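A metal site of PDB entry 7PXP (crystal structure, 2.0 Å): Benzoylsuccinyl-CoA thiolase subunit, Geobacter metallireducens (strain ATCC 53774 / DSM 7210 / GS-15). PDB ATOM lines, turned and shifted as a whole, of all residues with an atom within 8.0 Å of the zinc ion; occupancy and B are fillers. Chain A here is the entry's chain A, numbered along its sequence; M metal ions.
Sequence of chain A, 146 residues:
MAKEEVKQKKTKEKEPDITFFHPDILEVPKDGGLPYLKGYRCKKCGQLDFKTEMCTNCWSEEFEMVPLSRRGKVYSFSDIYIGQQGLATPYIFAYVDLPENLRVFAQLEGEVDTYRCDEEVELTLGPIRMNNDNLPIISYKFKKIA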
ATOM      1  N   ARG A  41     -23.668  13.765  31.386  1.00  0.00           N
ATOM      2  CA  ARG A  41     -23.261  13.433  30.037  1.00  0.00           C
ATOM      3  C   ARG A  41     -23.580  14.609  29.131  1.00  0.00           C
ATOM      4  O   ARG A  41     -24.714  15.103  29.121  1.00  0.00           O
ATOM      5  CB  ARG A  41     -23.920  12.137  29.540  1.00  0.00           C
ATOM      6  CG  ARG A  41     -23.361  11.660  28.188  1.00  0.00           C
ATOM      7  CD  ARG A  41     -23.769  10.247  27.834  1.00  0.00           C
ATOM      8  NE  ARG A  41     -22.910   9.315  28.559  1.00  0.00           N
ATOM      9  CZ  ARG A  41     -23.317   8.468  29.487  1.00  0.00           C
ATOM     10  NH1 ARG A  41     -24.619   8.367  29.774  1.00  0.00           N
ATOM     11  NH2 ARG A  41     -22.458   7.653  30.083  1.00  0.00           N
ATOM     12  N   CYS A  42     -22.571  15.065  28.387  1.00  0.00           N
ATOM     13  CA  CYS A  42     -22.751  16.147  27.430  1.00  0.00           C
ATOM     14  C   CYS A  42     -23.678  15.648  26.309  1.00  0.00           C
ATOM     15  O   CYS A  42     -23.450  14.569  25.766  1.00  0.00           O
ATOM     16  CB  CYS A  42     -21.421  16.646  26.887  1.00  0.00           C
ATOM     17  SG  CYS A  42     -21.578  17.899  25.602  1.00  0.00           S
ATOM     18  N   LYS A  43     -24.732  16.405  26.019  1.00  0.00           N
ATOM     19  CA  LYS A  43     -25.701  16.068  24.975  1.00  0.00           C
ATOM     20  C   LYS A  43     -25.111  16.226  23.554  1.00  0.00           C
ATOM     21  O   LYS A  43     -25.629  15.642  22.608  1.00  0.00           O
ATOM     22  CB  LYS A  43     -26.959  16.951  25.081  1.00  0.00           C
ATOM     23  CG  LYS A  43     -27.824  16.704  26.327  1.00  0.00           C
ATOM     24  CD  LYS A  43     -28.913  17.762  26.420  1.00  0.00           C
ATOM     25  CE  LYS A  43     -30.074  17.332  27.266  1.00  0.00           C
ATOM     26  NZ  LYS A  43     -31.228  18.264  27.112  1.00  0.00           N
ATOM     27  N   LYS A  44     -24.046  17.033  23.409  1.00  0.00           N
ATOM     28  CA  LYS A  44     -23.443  17.322  22.106  1.00  0.00           C
ATOM     29  C   LYS A  44     -22.327  16.337  21.713  1.00  0.00           C
ATOM     30  O   LYS A  44     -22.288  15.905  20.573  1.00  0.00           O
ATOM     31  CB  LYS A  44     -22.971  18.779  22.060  1.00  0.00           C
ATOM     32  CG  LYS A  44     -22.531  19.299  20.706  1.00  0.00           C
ATOM     33  CD  LYS A  44     -22.176  20.790  20.788  1.00  0.00           C
ATOM     34  CE  LYS A  44     -21.709  21.346  19.464  1.00  0.00           C
ATOM     35  NZ  LYS A  44     -20.379  20.822  19.063  1.00  0.00           N
ATOM     36  N   CYS A  45     -21.408  16.014  22.643  1.00  0.00           N
ATOM     37  CA  CYS A  45     -20.303  15.116  22.315  1.00  0.00           C
ATOM     38  C   CYS A  45     -20.377  13.738  23.021  1.00  0.00           C
ATOM     39  O   CYS A  45     -19.625  12.823  22.673  1.00  0.00           O
ATOM     40  CB  CYS A  45     -18.954  15.798  22.547  1.00  0.00           C
ATOM     41  SG  CYS A  45     -18.448  15.852  24.284  1.00  0.00           S
ATOM     42  N   GLY A  46     -21.279  13.606  23.985  1.00  0.00           N
ATOM     43  CA  GLY A  46     -21.462  12.351  24.718  1.00  0.00           C
ATOM     44  C   GLY A  46     -20.477  12.085  25.850  1.00  0.00           C
ATOM     45  O   GLY A  46     -20.502  10.994  26.429  1.00  0.00           O
ATOM     46  N   GLN A  47     -19.601  13.072  26.184  1.00  0.00           N
ATOM     47  CA  GLN A  47     -18.630  12.907  27.278  1.00  0.00           C
ATOM     48  C   GLN A  47     -19.310  12.908  28.626  1.00  0.00           C
ATOM     49  O   GLN A  47     -20.160  13.773  28.889  1.00  0.00           O
ATOM     50  CB  GLN A  47     -17.529  13.979  27.223  1.00  0.00           C
ATOM     51  CG  GLN A  47     -16.584  13.953  28.425  1.00  0.00           C
ATOM     52  CD  GLN A  47     -15.428  14.916  28.328  1.00  0.00           C
ATOM     53  OE1 GLN A  47     -14.372  14.588  27.798  1.00  0.00           O
ATOM     54  NE2 GLN A  47     -15.546  16.046  29.011  1.00  0.00           N
ATOM     55  N   LEU A  48     -18.948  11.940  29.486  1.00  0.00           N
ATOM     56  CA  LEU A  48     -19.420  11.827  30.860  1.00  0.00           C
ATOM     57  C   LEU A  48     -18.376  12.461  31.794  1.00  0.00           C
ATOM     58  O   LEU A  48     -17.177  12.213  31.645  1.00  0.00           O
ATOM     59  CB  LEU A  48     -19.657  10.357  31.253  1.00  0.00           C
ATOM     60  CG  LEU A  48     -20.195  10.097  32.685  1.00  0.00           C
ATOM     61  CD1 LEU A  48     -21.645  10.508  32.797  1.00  0.00           C
ATOM     62  CD2 LEU A  48     -20.001   8.630  33.088  1.00  0.00           C
ATOM     63  N   MET A  54     -19.733  24.136  31.530  1.00  0.00           N
ATOM     64  CA  MET A  54     -19.496  23.833  30.113  1.00  0.00           C
ATOM     65  C   MET A  54     -18.624  22.591  29.921  1.00  0.00           C
ATOM     66  O   MET A  54     -17.762  22.305  30.743  1.00  0.00           O
ATOM     67  CB  MET A  54     -18.943  25.048  29.334  1.00  0.00           C
ATOM     68  CG  MET A  54     -17.579  25.540  29.805  1.00  0.00           C
ATOM     69  SD  MET A  54     -16.648  26.541  28.606  1.00  0.00           S
ATOM     70  CE  MET A  54     -17.924  26.985  27.478  1.00  0.00           C
ATOM     71  N   CYS A  55     -18.885  21.854  28.829  1.00  0.00           N
ATOM     72  CA  CYS A  55     -18.173  20.621  28.516  1.00  0.00           C
ATOM     73  C   CYS A  55     -16.708  20.918  28.195  1.00  0.00           C
ATOM     74  O   CYS A  55     -16.427  21.732  27.312  1.00  0.00           O
ATOM     75  CB  CYS A  55     -18.873  19.875  27.381  1.00  0.00           C
ATOM     76  SG  CYS A  55     -18.011  18.380  26.809  1.00  0.00           S
ATOM     77  N   THR A  56     -15.769  20.262  28.889  1.00  0.00           N
ATOM     78  CA  THR A  56     -14.333  20.463  28.669  1.00  0.00           C
ATOM     79  C   THR A  56     -13.891  20.009  27.286  1.00  0.00           C
ATOM     80  O   THR A  56     -12.915  20.525  26.760  1.00  0.00           O
ATOM     81  CB  THR A  56     -13.470  19.807  29.782  1.00  0.00           C
ATOM     82  OG1 THR A  56     -13.619  18.395  29.694  1.00  0.00           O
ATOM     83  CG2 THR A  56     -13.812  20.321  31.199  1.00  0.00           C
ATOM     84  N   ASN A  57     -14.635  19.047  26.689  1.00  0.00           N
ATOM     85  CA  ASN A  57     -14.323  18.523  25.359  1.00  0.00           C
ATOM     86  C   ASN A  57     -14.832  19.393  24.189  1.00  0.00           C
ATOM     87  O   ASN A  57     -14.077  19.630  23.245  1.00  0.00           O
ATOM     88  CB  ASN A  57     -14.844  17.080  25.228  1.00  0.00           C
ATOM     89  CG  ASN A  57     -14.435  16.392  23.935  1.00  0.00           C
ATOM     90  OD1 ASN A  57     -13.242  16.204  23.645  1.00  0.00           O
ATOM     91  ND2 ASN A  57     -15.409  16.021  23.138  1.00  0.00           N
ATOM     92  N   CYS A  58     -16.102  19.839  24.242  1.00  0.00           N
ATOM     93  CA  CYS A  58     -16.689  20.555  23.110  1.00  0.00           C
ATOM     94  C   CYS A  58     -17.245  21.945  23.438  1.00  0.00           C
ATOM     95  O   CYS A  58     -17.665  22.658  22.521  1.00  0.00           O
ATOM     96  CB  CYS A  58     -17.732  19.687  22.403  1.00  0.00           C
ATOM     97  SG  CYS A  58     -19.328  19.645  23.249  1.00  0.00           S
ATOM     98  N   TRP A  59     -17.257  22.313  24.740  1.00  0.00           N
ATOM     99  CA  TRP A  59     -17.726  23.620  25.237  1.00  0.00           C
ATOM    100  C   TRP A  59     -19.256  23.804  25.238  1.00  0.00           C
ATOM    101  O   TRP A  59     -19.733  24.913  25.502  1.00  0.00           O
ATOM    102  CB  TRP A  59     -17.038  24.800  24.500  1.00  0.00           C
ATOM    103  CG  TRP A  59     -15.545  24.825  24.609  1.00  0.00           C
ATOM    104  CD1 TRP A  59     -14.754  24.053  25.417  1.00  0.00           C
ATOM    105  CD2 TRP A  59     -14.658  25.696  23.905  1.00  0.00           C
ATOM    106  NE1 TRP A  59     -13.436  24.390  25.254  1.00  0.00           N
ATOM    107  CE2 TRP A  59     -13.351  25.421  24.360  1.00  0.00           C
ATOM    108  CE3 TRP A  59     -14.851  26.708  22.938  1.00  0.00           C
ATOM    109  CZ2 TRP A  59     -12.244  26.148  23.913  1.00  0.00           C
ATOM    110  CZ3 TRP A  59     -13.749  27.422  22.495  1.00  0.00           C
ATOM    111  CH2 TRP A  59     -12.460  27.127  22.963  1.00  0.00           C
ATOM    112  N   SER A  60     -20.013  22.721  25.020  1.00  0.00           N
ATOM    113  CA  SER A  60     -21.470  22.792  25.060  1.00  0.00           C
ATOM    114  C   SER A  60     -21.911  23.000  26.510  1.00  0.00           C
ATOM    115  O   SER A  60     -21.173  22.657  27.441  1.00  0.00           O
ATOM    116  CB  SER A  60     -22.083  21.501  24.509  1.00  0.00           C
ATOM    117  OG  SER A  60     -23.479  21.438  24.745  1.00  0.00           O
ATOM    118  N   GLU A  61     -23.099  23.582  26.725  1.00  0.00           N
ATOM    119  CA  GLU A  61     -23.631  23.846  28.053  1.00  0.00           C
ATOM    120  C   GLU A  61     -24.895  23.002  28.334  1.00  0.00           C
ATOM    121  O   GLU A  61     -25.580  23.223  29.338  1.00  0.00           O
ATOM    122  CB  GLU A  61     -23.885  25.353  28.240  1.00  0.00           C
ATOM    123  CG  GLU A  61     -22.598  26.160  28.266  1.00  0.00           C
ATOM    124  CD  GLU A  61     -22.713  27.672  28.270  1.00  0.00           C
ATOM    125  OE1 GLU A  61     -23.672  28.212  28.861  1.00  0.00           O
ATOM    126  OE2 GLU A  61     -21.759  28.318  27.769  1.00  0.00           O
ATOM    127  N   GLU A  62     -25.159  22.009  27.449  1.00  0.00           N
ATOM    128  CA  GLU A  62     -26.326  21.123  27.511  1.00  0.00           C
ATOM    129  C   GLU A  62     -25.963  19.712  27.968  1.00  0.00           C
ATOM    130  O   GLU A  62     -25.217  19.008  27.298  1.00  0.00           O
ATOM    131  CB  GLU A  62     -27.071  21.103  26.158  1.00  0.00           C
ATOM    132  CG  GLU A  62     -27.670  22.440  25.737  1.00  0.00           C
ATOM    133  CD  GLU A  62     -28.505  23.176  26.777  1.00  0.00           C
ATOM    134  OE1 GLU A  62     -29.405  22.551  27.388  1.00  0.00           O
ATOM    135  OE2 GLU A  62     -28.243  24.385  26.988  1.00  0.00           O
ATOM    136  N   PHE A  63     -26.487  19.311  29.146  1.00  0.00           N
ATOM    137  CA  PHE A  63     -26.179  18.028  29.767  1.00  0.00           C
ATOM    138  C   PHE A  63     -27.412  17.251  30.227  1.00  0.00           C
ATOM    139  O   PHE A  63     -28.481  17.828  30.416  1.00  0.00           O
ATOM    140  CB  PHE A  63     -25.222  18.241  30.979  1.00  0.00           C
ATOM    141  CG  PHE A  63     -24.014  19.134  30.750  1.00  0.00           C
ATOM    142  CD1 PHE A  63     -22.827  18.606  30.268  1.00  0.00           C
ATOM    143  CD2 PHE A  63     -24.072  20.486  31.057  1.00  0.00           C
ATOM    144  CE1 PHE A  63     -21.709  19.439  30.076  1.00  0.00           C
ATOM    145  CE2 PHE A  63     -22.952  21.311  30.842  1.00  0.00           C
ATOM    146  CZ  PHE A  63     -21.786  20.777  30.360  1.00  0.00           C
HETATM  147 ZN    ZN M   1     -19.290  17.869  25.025  1.00  0.00          ZN
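Within 4 Å of the zinc ion: Cys 42, Cys 45, Cys 55 and Cys 58. Along chain A the residues within 4 Å of the zinc ion span positions 42 to 58.
SG of Cys 55 sits close to N of Asn 57. The backbone NH (N) of Cys 55 is in hydrogen-bond range of the backbone carbonyl oxygen (O) of Ser 60 (2.8 Å). The side-chain sulfur (SG) of Cys 45 sits close to the side-chain amide nitrogen (ND2) of Asn 57 (3.3 Å). N of Gln 47 lies close to SG of Cys 45 (3.6 Å). The backbone NH of Lys 44 sits close to the side-chain sulfur of Cys 42, 3.4 Å away. The backbone NH (N) of Cys 42 lies within hydrogen-bond range of the backbone carbonyl oxygen (O) of Gln 47 (2.8 Å). N of Ser 60 lies close to SG of Cys 58.
The zinc ion is bound by the side-chain sulfur (SG) of Cys 55 (2.3 Å). The zinc ion is bound by SG of Cys 45, at 2.3 Å. The side-chain sulfur (SG) of Cys 42 is bound to the zinc ion. SG of Cys 58 binds the zinc ion, 2.5 Å away. The zinc ion has four donor atoms within binding distance.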
